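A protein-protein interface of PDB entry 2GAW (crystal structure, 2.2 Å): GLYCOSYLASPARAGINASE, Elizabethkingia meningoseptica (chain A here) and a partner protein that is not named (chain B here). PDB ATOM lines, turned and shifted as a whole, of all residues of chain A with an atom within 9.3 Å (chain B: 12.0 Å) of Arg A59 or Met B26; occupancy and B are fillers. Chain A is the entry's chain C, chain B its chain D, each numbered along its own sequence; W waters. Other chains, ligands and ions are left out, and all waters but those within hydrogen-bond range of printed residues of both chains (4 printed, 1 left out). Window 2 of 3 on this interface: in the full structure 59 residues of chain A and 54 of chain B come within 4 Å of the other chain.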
ATOM      1  N   ARG A  56     -24.608  17.812  21.101  1.00  0.00           N
ATOM      2  CA  ARG A  56     -23.960  16.675  21.723  1.00  0.00           C
ATOM      3  C   ARG A  56     -22.905  17.128  22.731  1.00  0.00           C
ATOM      4  O   ARG A  56     -22.062  17.992  22.465  1.00  0.00           O
ATOM      5  CB  ARG A  56     -23.321  15.793  20.661  1.00  0.00           C
ATOM      6  CG  ARG A  56     -24.365  15.212  19.742  1.00  0.00           C
ATOM      7  CD  ARG A  56     -23.629  14.735  18.526  1.00  0.00           C
ATOM      8  NE  ARG A  56     -24.532  14.307  17.474  1.00  0.00           N
ATOM      9  CZ  ARG A  56     -24.421  14.784  16.232  1.00  0.00           C
ATOM     10  NH1 ARG A  56     -23.475  15.687  15.910  1.00  0.00           N
ATOM     11  NH2 ARG A  56     -25.268  14.344  15.312  1.00  0.00           N
ATOM     12  N   PRO A  57     -22.977  16.593  23.946  1.00  0.00           N
ATOM     13  CA  PRO A  57     -22.143  16.978  25.065  1.00  0.00           C
ATOM     14  C   PRO A  57     -20.672  16.606  24.957  1.00  0.00           C
ATOM     15  O   PRO A  57     -20.219  15.932  24.014  1.00  0.00           O
ATOM     16  CB  PRO A  57     -22.868  16.338  26.212  1.00  0.00           C
ATOM     17  CG  PRO A  57     -23.343  15.023  25.643  1.00  0.00           C
ATOM     18  CD  PRO A  57     -23.931  15.563  24.356  1.00  0.00           C
ATOM     19  N   ASP A  58     -19.898  17.104  25.924  1.00  0.00           N
ATOM     20  CA  ASP A  58     -18.507  16.721  26.050  1.00  0.00           C
ATOM     21  C   ASP A  58     -18.496  15.288  26.590  1.00  0.00           C
ATOM     22  O   ASP A  58     -19.546  14.693  26.872  1.00  0.00           O
ATOM     23  CB  ASP A  58     -17.726  17.685  27.009  1.00  0.00           C
ATOM     24  CG  ASP A  58     -18.002  17.779  28.501  1.00  0.00           C
ATOM     25  OD1 ASP A  58     -18.578  16.887  29.113  1.00  0.00           O
ATOM     26  OD2 ASP A  58     -17.605  18.765  29.113  1.00  0.00           O
ATOM     27  N   ARG A  59     -17.306  14.728  26.772  1.00  0.00           N
ATOM     28  CA  ARG A  59     -17.165  13.350  27.173  1.00  0.00           C
ATOM     29  C   ARG A  59     -17.726  13.028  28.549  1.00  0.00           C
ATOM     30  O   ARG A  59     -18.063  11.858  28.797  1.00  0.00           O
ATOM     31  CB  ARG A  59     -15.692  12.949  27.109  1.00  0.00           C
ATOM     32  CG  ARG A  59     -14.743  13.606  28.075  1.00  0.00           C
ATOM     33  CD  ARG A  59     -13.450  12.885  27.860  1.00  0.00           C
ATOM     34  NE  ARG A  59     -12.478  13.359  28.823  1.00  0.00           N
ATOM     35  CZ  ARG A  59     -11.175  13.096  28.750  1.00  0.00           C
ATOM     36  NH1 ARG A  59     -10.697  12.342  27.749  1.00  0.00           N
ATOM     37  NH2 ARG A  59     -10.370  13.685  29.642  1.00  0.00           N
ATOM     38  N   ASP A  60     -17.909  14.046  29.395  1.00  0.00           N
ATOM     39  CA  ASP A  60     -18.471  13.836  30.718  1.00  0.00           C
ATOM     40  C   ASP A  60     -19.958  14.156  30.700  1.00  0.00           C
ATOM     41  O   ASP A  60     -20.620  14.248  31.737  1.00  0.00           O
ATOM     42  CB  ASP A  60     -17.771  14.728  31.744  1.00  0.00           C
ATOM     43  CG  ASP A  60     -16.244  14.709  31.752  1.00  0.00           C
ATOM     44  OD1 ASP A  60     -15.621  13.658  31.666  1.00  0.00           O
ATOM     45  OD2 ASP A  60     -15.651  15.787  31.855  1.00  0.00           O
ATOM     46  N   GLY A  61     -20.536  14.343  29.513  1.00  0.00           N
ATOM     47  CA  GLY A  61     -21.960  14.601  29.364  1.00  0.00           C
ATOM     48  C   GLY A  61     -22.386  16.044  29.550  1.00  0.00           C
ATOM     49  O   GLY A  61     -23.591  16.307  29.543  1.00  0.00           O
ATOM     50  N   ARG A  62     -21.467  17.012  29.639  1.00  0.00           N
ATOM     51  CA  ARG A  62     -21.838  18.409  29.811  1.00  0.00           C
ATOM     52  C   ARG A  62     -22.054  19.092  28.472  1.00  0.00           C
ATOM     53  O   ARG A  62     -21.242  18.941  27.556  1.00  0.00           O
ATOM     54  CB  ARG A  62     -20.757  19.145  30.557  1.00  0.00           C
ATOM     55  CG  ARG A  62     -20.576  18.660  31.981  1.00  0.00           C
ATOM     56  CD  ARG A  62     -19.525  19.585  32.585  1.00  0.00           C
ATOM     57  NE  ARG A  62     -18.569  18.927  33.473  1.00  0.00           N
ATOM     58  CZ  ARG A  62     -17.655  18.043  33.031  1.00  0.00           C
ATOM     59  NH1 ARG A  62     -17.586  17.715  31.731  1.00  0.00           N
ATOM     60  NH2 ARG A  62     -16.713  17.555  33.861  1.00  0.00           N
ATOM     61  N   VAL A  63     -23.129  19.858  28.284  1.00  0.00           N
ATOM     62  CA  VAL A  63     -23.347  20.513  27.006  1.00  0.00           C
ATOM     63  C   VAL A  63     -22.697  21.866  27.213  1.00  0.00           C
ATOM     64  O   VAL A  63     -23.049  22.629  28.107  1.00  0.00           O
ATOM     65  CB  VAL A  63     -24.849  20.678  26.678  1.00  0.00           C
ATOM     66  CG1 VAL A  63     -25.010  21.313  25.294  1.00  0.00           C
ATOM     67  CG2 VAL A  63     -25.529  19.320  26.676  1.00  0.00           C
ATOM     68  N   THR A  64     -21.732  22.154  26.362  1.00  0.00           N
ATOM     69  CA  THR A  64     -20.911  23.335  26.492  1.00  0.00           C
ATOM     70  C   THR A  64     -20.867  23.944  25.107  1.00  0.00           C
ATOM     71  O   THR A  64     -20.490  23.277  24.129  1.00  0.00           O
ATOM     72  CB  THR A  64     -19.618  22.740  27.049  1.00  0.00           C
ATOM     73  OG1 THR A  64     -19.749  22.860  28.460  1.00  0.00           O
ATOM     74  CG2 THR A  64     -18.347  23.336  26.477  1.00  0.00           C
ATOM     75  N   ASP A  66     -20.134  27.381  22.457  1.00  0.00           N
ATOM     76  CA  ASP A  66     -19.182  28.409  22.081  1.00  0.00           C
ATOM     77  C   ASP A  66     -19.816  29.279  21.000  1.00  0.00           C
ATOM     78  O   ASP A  66     -20.511  28.762  20.107  1.00  0.00           O
ATOM     79  CB  ASP A  66     -17.891  27.816  21.496  1.00  0.00           C
ATOM     80  CG  ASP A  66     -17.234  26.645  22.222  1.00  0.00           C
ATOM     81  OD1 ASP A  66     -17.180  26.592  23.441  1.00  0.00           O
ATOM     82  OD2 ASP A  66     -16.752  25.740  21.545  1.00  0.00           O
ATOM     83  N   CYS A  81     -17.307  27.702  26.070  1.00  0.00           N
ATOM     84  CA  CYS A  81     -17.524  26.638  27.045  1.00  0.00           C
ATOM     85  C   CYS A  81     -18.507  27.125  28.104  1.00  0.00           C
ATOM     86  O   CYS A  81     -18.214  27.294  29.290  1.00  0.00           O
ATOM     87  CB  CYS A  81     -16.161  26.212  27.669  1.00  0.00           C
ATOM     88  SG  CYS A  81     -16.212  24.791  28.810  1.00  0.00           S
ATOM     89  N   GLU A 131     -27.373   8.822  23.268  1.00  0.00           N
ATOM     90  CA  GLU A 131     -26.201   8.646  22.421  1.00  0.00           C
ATOM     91  C   GLU A 131     -24.900   8.801  23.186  1.00  0.00           C
ATOM     92  O   GLU A 131     -23.953   8.043  22.938  1.00  0.00           O
ATOM     93  CB  GLU A 131     -26.175   9.653  21.268  1.00  0.00           C
ATOM     94  CG  GLU A 131     -27.120   9.297  20.155  1.00  0.00           C
ATOM     95  CD  GLU A 131     -27.189  10.225  18.959  1.00  0.00           C
ATOM     96  OE1 GLU A 131     -26.322  11.086  18.747  1.00  0.00           O
ATOM     97  OE2 GLU A 131     -28.173  10.160  18.231  1.00  0.00           O
ATOM     98  N   TRP A 132     -24.792   9.750  24.121  1.00  0.00           N
ATOM     99  CA  TRP A 132     -23.595   9.875  24.933  1.00  0.00           C
ATOM    100  C   TRP A 132     -23.396   8.579  25.710  1.00  0.00           C
ATOM    101  O   TRP A 132     -22.287   8.036  25.745  1.00  0.00           O
ATOM    102  CB  TRP A 132     -23.735  11.093  25.875  1.00  0.00           C
ATOM    103  CG  TRP A 132     -22.694  11.184  26.988  1.00  0.00           C
ATOM    104  CD1 TRP A 132     -21.346  11.203  26.746  1.00  0.00           C
ATOM    105  CD2 TRP A 132     -22.989  11.200  28.319  1.00  0.00           C
ATOM    106  NE1 TRP A 132     -20.782  11.213  27.921  1.00  0.00           N
ATOM    107  CE2 TRP A 132     -21.710  11.209  28.885  1.00  0.00           C
ATOM    108  CE3 TRP A 132     -24.127  11.198  29.123  1.00  0.00           C
ATOM    109  CZ2 TRP A 132     -21.550  11.219  30.273  1.00  0.00           C
ATOM    110  CZ3 TRP A 132     -23.963  11.210  30.508  1.00  0.00           C
ATOM    111  CH2 TRP A 132     -22.689  11.221  31.082  1.00  0.00           C
ATOM    112  N   LYS A 133     -24.461   8.022  26.274  1.00  0.00           N
ATOM    113  CA  LYS A 133     -24.362   6.764  26.986  1.00  0.00           C
ATOM    114  C   LYS A 133     -24.121   5.568  26.063  1.00  0.00           C
ATOM    115  O   LYS A 133     -23.881   4.434  26.517  1.00  0.00           O
ATOM    116  CB  LYS A 133     -25.628   6.559  27.802  1.00  0.00           C
ATOM    117  CG  LYS A 133     -25.614   7.497  29.006  1.00  0.00           C
ATOM    118  CD  LYS A 133     -26.924   7.481  29.778  1.00  0.00           C
ATOM    119  CE  LYS A 133     -26.803   8.348  31.023  1.00  0.00           C
ATOM    120  NZ  LYS A 133     -28.108   8.721  31.535  1.00  0.00           N
ATOM    121  N   TRP A 135     -21.940   5.969  23.359  1.00  0.00           N
ATOM    122  CA  TRP A 135     -20.527   6.265  23.202  1.00  0.00           C
ATOM    123  C   TRP A 135     -19.738   5.844  24.445  1.00  0.00           C
ATOM    124  O   TRP A 135     -18.629   5.326  24.312  1.00  0.00           O
ATOM    125  CB  TRP A 135     -20.347   7.767  22.941  1.00  0.00           C
ATOM    126  CG  TRP A 135     -18.889   8.182  22.770  1.00  0.00           C
ATOM    127  CD1 TRP A 135     -18.231   8.019  21.579  1.00  0.00           C
ATOM    128  CD2 TRP A 135     -18.091   8.719  23.755  1.00  0.00           C
ATOM    129  NE1 TRP A 135     -17.011   8.442  21.811  1.00  0.00           N
ATOM    130  CE2 TRP A 135     -16.877   8.866  23.077  1.00  0.00           C
ATOM    131  CE3 TRP A 135     -18.214   9.089  25.093  1.00  0.00           C
ATOM    132  CZ2 TRP A 135     -15.762   9.386  23.736  1.00  0.00           C
ATOM    133  CZ3 TRP A 135     -17.097   9.612  25.747  1.00  0.00           C
ATOM    134  CH2 TRP A 135     -15.880   9.759  25.076  1.00  0.00           C
ATOM    135  N   LEU A 136     -20.270   6.010  25.655  1.00  0.00           N
ATOM    136  CA  LEU A 136     -19.570   5.599  26.860  1.00  0.00           C
ATOM    137  C   LEU A 136     -19.290   4.098  26.904  1.00  0.00           C
ATOM    138  O   LEU A 136     -18.338   3.667  27.558  1.00  0.00           O
ATOM    139  CB  LEU A 136     -20.365   5.974  28.104  1.00  0.00           C
ATOM    140  CG  LEU A 136     -20.529   7.441  28.509  1.00  0.00           C
ATOM    141  CD1 LEU A 136     -21.450   7.517  29.715  1.00  0.00           C
ATOM    142  CD2 LEU A 136     -19.183   8.057  28.852  1.00  0.00           C
ATOM    143  N   LYS A 137     -20.101   3.282  26.222  1.00  0.00           N
ATOM    144  CA  LYS A 137     -19.879   1.846  26.191  1.00  0.00           C
ATOM    145  C   LYS A 137     -18.796   1.569  25.165  1.00  0.00           C
ATOM    146  O   LYS A 137     -17.844   0.832  25.408  1.00  0.00           O
ATOM    147  CB  LYS A 137     -21.122   1.092  25.772  1.00  0.00           C
ATOM    148  CG  LYS A 137     -22.320   1.373  26.646  1.00  0.00           C
ATOM    149  CD  LYS A 137     -23.449   0.501  26.126  1.00  0.00           C
ATOM    150  CE  LYS A 137     -24.767   0.824  26.819  1.00  0.00           C
ATOM    151  NZ  LYS A 137     -25.313   2.074  26.319  1.00  0.00           N
ATOM    152  N   THR B  19     -21.822  27.075  18.116  1.00  0.00           N
ATOM    153  CA  THR B  19     -21.604  25.637  18.156  1.00  0.00           C
ATOM    154  C   THR B  19     -21.766  25.062  19.563  1.00  0.00           C
ATOM    155  O   THR B  19     -21.772  25.776  20.571  1.00  0.00           O
ATOM    156  CB  THR B  19     -20.177  25.336  17.619  1.00  0.00           C
ATOM    157  OG1 THR B  19     -20.084  23.935  17.370  1.00  0.00           O
ATOM    158  CG2 THR B  19     -19.100  25.742  18.598  1.00  0.00           C
ATOM    159  N   SER B  20     -21.973  23.740  19.579  1.00  0.00           N
ATOM    160  CA  SER B  20     -21.879  22.931  20.779  1.00  0.00           C
ATOM    161  C   SER B  20     -20.536  22.181  20.708  1.00  0.00           C
ATOM    162  O   SER B  20     -20.121  21.456  21.625  1.00  0.00           O
ATOM    163  CB  SER B  20     -23.049  21.956  20.843  1.00  0.00           C
ATOM    164  OG  SER B  20     -23.215  21.104  19.722  1.00  0.00           O
ATOM    165  N   GLY B  21     -19.802  22.374  19.604  1.00  0.00           N
ATOM    166  CA  GLY B  21     -18.471  21.826  19.416  1.00  0.00           C
ATOM    167  C   GLY B  21     -18.437  20.339  19.107  1.00  0.00           C
ATOM    168  O   GLY B  21     -19.441  19.693  18.802  1.00  0.00           O
ATOM    169  N   MET B  22     -17.206  19.833  19.174  1.00  0.00           N
ATOM    170  CA  MET B  22     -16.932  18.421  18.923  1.00  0.00           C
ATOM    171  C   MET B  22     -17.631  17.534  19.940  1.00  0.00           C
ATOM    172  O   MET B  22     -17.550  17.760  21.150  1.00  0.00           O
ATOM    173  CB  MET B  22     -15.449  18.149  19.004  1.00  0.00           C
ATOM    174  CG  MET B  22     -15.091  16.729  18.553  1.00  0.00           C
ATOM    175  SD  MET B  22     -13.388  16.285  18.957  1.00  0.00           S
ATOM    176  CE  MET B  22     -12.589  17.703  18.255  1.00  0.00           C
ATOM    177  N   ALA B  23     -18.327  16.531  19.442  1.00  0.00           N
ATOM    178  CA  ALA B  23     -19.015  15.607  20.301  1.00  0.00           C
ATOM    179  C   ALA B  23     -18.010  14.758  21.068  1.00  0.00           C
ATOM    180  O   ALA B  23     -17.059  14.189  20.531  1.00  0.00           O
ATOM    181  CB  ALA B  23     -19.896  14.693  19.475  1.00  0.00           C
ATOM    182  N   TYR B  24     -18.293  14.703  22.367  1.00  0.00           N
ATOM    183  CA  TYR B  24     -17.562  13.948  23.366  1.00  0.00           C
ATOM    184  C   TYR B  24     -16.126  14.412  23.479  1.00  0.00           C
ATOM    185  O   TYR B  24     -15.192  13.684  23.776  1.00  0.00           O
ATOM    186  CB  TYR B  24     -17.648  12.448  23.038  1.00  0.00           C
ATOM    187  CG  TYR B  24     -19.065  12.032  22.683  1.00  0.00           C
ATOM    188  CD1 TYR B  24     -20.125  12.380  23.517  1.00  0.00           C
ATOM    189  CD2 TYR B  24     -19.304  11.373  21.465  1.00  0.00           C
ATOM    190  CE1 TYR B  24     -21.429  12.083  23.134  1.00  0.00           C
ATOM    191  CE2 TYR B  24     -20.621  11.067  21.080  1.00  0.00           C
ATOM    192  CZ  TYR B  24     -21.670  11.435  21.924  1.00  0.00           C
ATOM    193  OH  TYR B  24     -22.971  11.189  21.556  1.00  0.00           O
ATOM    194  N   LYS B  25     -15.979  15.722  23.286  1.00  0.00           N
ATOM    195  CA  LYS B  25     -14.722  16.451  23.460  1.00  0.00           C
ATOM    196  C   LYS B  25     -14.282  16.383  24.927  1.00  0.00           C
ATOM    197  O   LYS B  25     -15.048  16.002  25.815  1.00  0.00           O
ATOM    198  CB  LYS B  25     -14.946  17.921  23.025  1.00  0.00           C
ATOM    199  CG  LYS B  25     -16.014  18.590  23.907  1.00  0.00           C
ATOM    200  CD  LYS B  25     -16.570  19.885  23.352  1.00  0.00           C
ATOM    201  CE  LYS B  25     -17.722  20.361  24.224  1.00  0.00           C
ATOM    202  NZ  LYS B  25     -18.499  21.407  23.586  1.00  0.00           N
ATOM    203  N   MET B  26     -13.048  16.781  25.239  1.00  0.00           N
ATOM    204  CA  MET B  26     -12.595  16.848  26.627  1.00  0.00           C
ATOM    205  C   MET B  26     -13.309  18.029  27.250  1.00  0.00           C
ATOM    206  O   MET B  26     -13.628  19.001  26.550  1.00  0.00           O
ATOM    207  CB  MET B  26     -11.110  17.120  26.743  1.00  0.00           C
ATOM    208  CG  MET B  26     -10.259  15.890  26.765  1.00  0.00           C
ATOM    209  SD  MET B  26      -8.516  16.366  26.778  1.00  0.00           S
ATOM    210  CE  MET B  26      -8.312  16.762  28.488  1.00  0.00           C
ATOM    211  N   HIS B  27     -13.554  17.982  28.546  1.00  0.00           N
ATOM    212  CA  HIS B  27     -14.237  19.082  29.186  1.00  0.00           C
ATOM    213  C   HIS B  27     -13.414  20.358  29.080  1.00  0.00           C
ATOM    214  O   HIS B  27     -12.197  20.345  29.252  1.00  0.00           O
ATOM    215  CB  HIS B  27     -14.500  18.748  30.656  1.00  0.00           C
ATOM    216  CG  HIS B  27     -15.283  19.837  31.382  1.00  0.00           C
ATOM    217  ND1 HIS B  27     -16.263  20.621  30.930  1.00  0.00           N
ATOM    218  CD2 HIS B  27     -15.039  20.195  32.677  1.00  0.00           C
ATOM    219  CE1 HIS B  27     -16.613  21.437  31.890  1.00  0.00           C
ATOM    220  NE2 HIS B  27     -15.863  21.166  32.939  1.00  0.00           N
ATOM    221  N   GLY B  28     -14.075  21.447  28.712  1.00  0.00           N
ATOM    222  CA  GLY B  28     -13.420  22.728  28.617  1.00  0.00           C
ATOM    223  C   GLY B  28     -12.799  22.956  27.256  1.00  0.00           C
ATOM    224  O   GLY B  28     -12.207  24.009  27.036  1.00  0.00           O
ATOM    225  N   ARG B  29     -12.894  22.004  26.339  1.00  0.00           N
ATOM    226  CA  ARG B  29     -12.363  22.153  24.993  1.00  0.00           C
ATOM    227  C   ARG B  29     -13.109  23.255  24.257  1.00  0.00           C
ATOM    228  O   ARG B  29     -14.338  23.324  24.370  1.00  0.00           O
ATOM    229  CB  ARG B  29     -12.528  20.828  24.255  1.00  0.00           C
ATOM    230  CG  ARG B  29     -11.989  20.748  22.830  1.00  0.00           C
ATOM    231  CD  ARG B  29     -13.066  21.119  21.833  1.00  0.00           C
ATOM    232  NE  ARG B  29     -12.586  21.039  20.484  1.00  0.00           N
ATOM    233  CZ  ARG B  29     -13.278  21.534  19.461  1.00  0.00           C
ATOM    234  NH1 ARG B  29     -14.454  22.150  19.619  1.00  0.00           N
ATOM    235  NH2 ARG B  29     -12.775  21.402  18.248  1.00  0.00           N
ATOM    236  N   VAL B  30     -12.415  24.112  23.505  1.00  0.00           N
ATOM    237  CA  VAL B  30     -13.110  25.074  22.670  1.00  0.00           C
ATOM    238  C   VAL B  30     -12.406  24.952  21.328  1.00  0.00           C
ATOM    239  O   VAL B  30     -11.240  24.528  21.227  1.00  0.00           O
ATOM    240  CB  VAL B  30     -13.067  26.611  23.183  1.00  0.00           C
ATOM    241  CG1 VAL B  30     -12.968  26.619  24.699  1.00  0.00           C
ATOM    242  CG2 VAL B  30     -11.964  27.425  22.575  1.00  0.00           C
ATOM    243  N   GLY B  31     -13.184  25.227  20.289  1.00  0.00           N
ATOM    244  CA  GLY B  31     -12.677  25.212  18.937  1.00  0.00           C
ATOM    245  C   GLY B  31     -12.634  26.641  18.435  1.00  0.00           C
ATOM    246  O   GLY B  31     -12.604  27.599  19.213  1.00  0.00           O
ATOM    247  N   GLU B  56      -9.654  22.689  15.678  1.00  0.00           N
ATOM    248  CA  GLU B  56      -8.229  22.730  15.977  1.00  0.00           C
ATOM    249  C   GLU B  56      -7.388  23.254  14.816  1.00  0.00           C
ATOM    250  O   GLU B  56      -6.510  24.110  14.966  1.00  0.00           O
ATOM    251  CB  GLU B  56      -7.771  21.310  16.363  1.00  0.00           C
ATOM    252  CG  GLU B  56      -8.191  20.789  17.756  1.00  0.00           C
ATOM    253  CD  GLU B  56      -9.679  20.625  18.054  1.00  0.00           C
ATOM    254  OE1 GLU B  56     -10.501  20.420  17.155  1.00  0.00           O
ATOM    255  OE2 GLU B  56     -10.060  20.741  19.218  1.00  0.00           O
ATOM    256  N   ILE B  59      -8.120  27.012  14.151  1.00  0.00           N
ATOM    257  CA  ILE B  59      -7.398  27.819  15.131  1.00  0.00           C
ATOM    258  C   ILE B  59      -5.947  27.946  14.683  1.00  0.00           C
ATOM    259  O   ILE B  59      -5.442  29.063  14.518  1.00  0.00           O
ATOM    260  CB  ILE B  59      -7.459  27.166  16.554  1.00  0.00           C
ATOM    261  CG1 ILE B  59      -8.891  27.170  17.075  1.00  0.00           C
ATOM    262  CG2 ILE B  59      -6.599  27.962  17.538  1.00  0.00           C
ATOM    263  CD1 ILE B  59      -9.103  26.519  18.452  1.00  0.00           C
HETATM  264  O   HOH W   1     -14.421  23.757  31.583  1.00  0.00           O
HETATM  265  O   HOH W   2     -12.892  15.545  30.473  1.00  0.00           O
HETATM  266  O   HOH W   3     -16.759  21.060  27.857  1.00  0.00           O
HETATM  267  O   HOH W   4     -15.777  25.693  18.866  1.00  0.00           O
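Of chain B, only Tyr B24, Lys B25 and Met B26 come within 4 Å of Arg A59. Met B26 touches one residue of chain A. Of the printed residues of chain B, Pro A57 touches Ala B23 and Tyr B24. Asp A58 touches three residues of chain B. Asp A60 touches just one residue of chain B: His B27 (3.4 Å). Of the printed residues of chain A, Ala B23 touches Arg A56 (3.8 Å) and Pro A57 (3.9 Å). Of the printed residues of chain A, Gly B31 touches Asp A66. Printed residues of chain B within 4 Å of Thr A64: Ser B20 and Lys B25. Printed residues of chain A within 4 Å of Tyr B24: Pro A57, Asp A58, Arg A59, Glu A131, Trp A132 and Trp A135. Val A63 touches none of the printed residues of chain B. The nearest printed residue of chain B that does not touch Cys A81 is Val B30 (4.4 Å).
Of the 17 printed residues of chain A, 12 touch a printed residue of chain B. Hydrophobic or aromatic side chains of chain A that line the printed part of chain B: Trp A132 and Trp A135. Along chain A the printed residues that touch a printed residue of chain B span positions 56 to 135. Among the printed residues, 21 pairs touch across the chains. Among the printed residues, no Asp or Glu carboxylate lies within 4 Å of a Lys or Arg side-chain nitrogen of the other chain.
The guanidinium group (NE) of Arg A56 is in salt-bridge range of the side-chain carboxylate (OE1) of Glu A131, at 3.9 Å. The backbone NH (N) of Asp A60 is in hydrogen-bond range of the side-chain carboxylate (OD1) of Asp A58, at 2.9 Å. OD1 of Asp A58 sits at hydrogen-bond distance from N of Gly A61, at 3.2 Å. OD2 of Asp A58 lies within salt-bridge range of NH1 of Arg A62 (2.8 Å). OD1 of Asp A66 sits at hydrogen-bond distance from N of Cys A81 (2.9 Å). OG1 of Thr B19 is in hydrogen-bond range of N of Gly B21, 2.7 Å away.
O of Pro A57 sits at hydrogen-bond distance from N of Tyr B24, at 2.8 Å. The side-chain carboxylate (OD2) of Asp A58 is in hydrogen-bond range of a ring nitrogen (ND1) of His B27, 2.9 Å away. The backbone NH (N) of Arg A59 lies within hydrogen-bond range of the backbone carbonyl oxygen (O) of Lys B25 (2.8 Å). The guanidinium group (NH1) of Arg A62 lies close to a ring nitrogen (ND1) of His B27. The side-chain amino group (NZ) of Lys B25 sits at hydrogen-bond distance from the backbone carbonyl oxygen (O) of Thr A64. The backbone carbonyl oxygen (O) of Asp A66 is in hydrogen-bond range of the backbone NH (N) of Thr B19, at 2.9 Å. The backbone NH of Trp A132 lies within hydrogen-bond range of the side-chain hydroxyl of Tyr B24 (3.5 Å). The backbone carbonyl oxygen of Thr A64 sits close to the backbone carbonyl oxygen of Ser B20, at 3.1 Å.
Arg A56 touches Ser B20. Arg A56 touches Ala B23. Ala B23 touches Pro A57 (C to O, 3.9 Å). CA of Tyr B24 touches C of Asp A58, at 3.6 Å. CG of Met B26 touches CZ of Arg A59, at 3.5 Å. His B27 touches Asp A60 (CB to OD2, 3.4 Å). Asp A66 touches Val B30 (OD2 to CA, 3.9 Å). Gly B31 touches Asp A66 (N to OD2, 3.8 Å). Glu A131 touches Tyr B24 (C to OH, 3.5 Å). Trp A135 touches Tyr B24 (CG to CD2, 3.5 Å).
Water W3 lies within hydrogen-bond range of the side-chain carboxylate (OD2) of Asp A58 (2.7 Å), the backbone NH (N) of Gly B28 (2.8 Å) and a ring nitrogen (ND1) of His B27 (3.1 Å). Water W2 lies within hydrogen-bond range of the guanidinium group (NE) of Arg A59 (2.8 Å), the side-chain carboxylate (OD2) of Asp A60 (3.1 Å) and the backbone NH (N) of His B27 (3.2 Å). Water W4 lies within hydrogen-bond range of OD2 of Asp A66 (2.9 Å) and N of Gly B31 (3.0 Å). Water W1 bridges NE2 of His B27 (3.3 Å) and SG of Cys A81 (3.5 Å).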
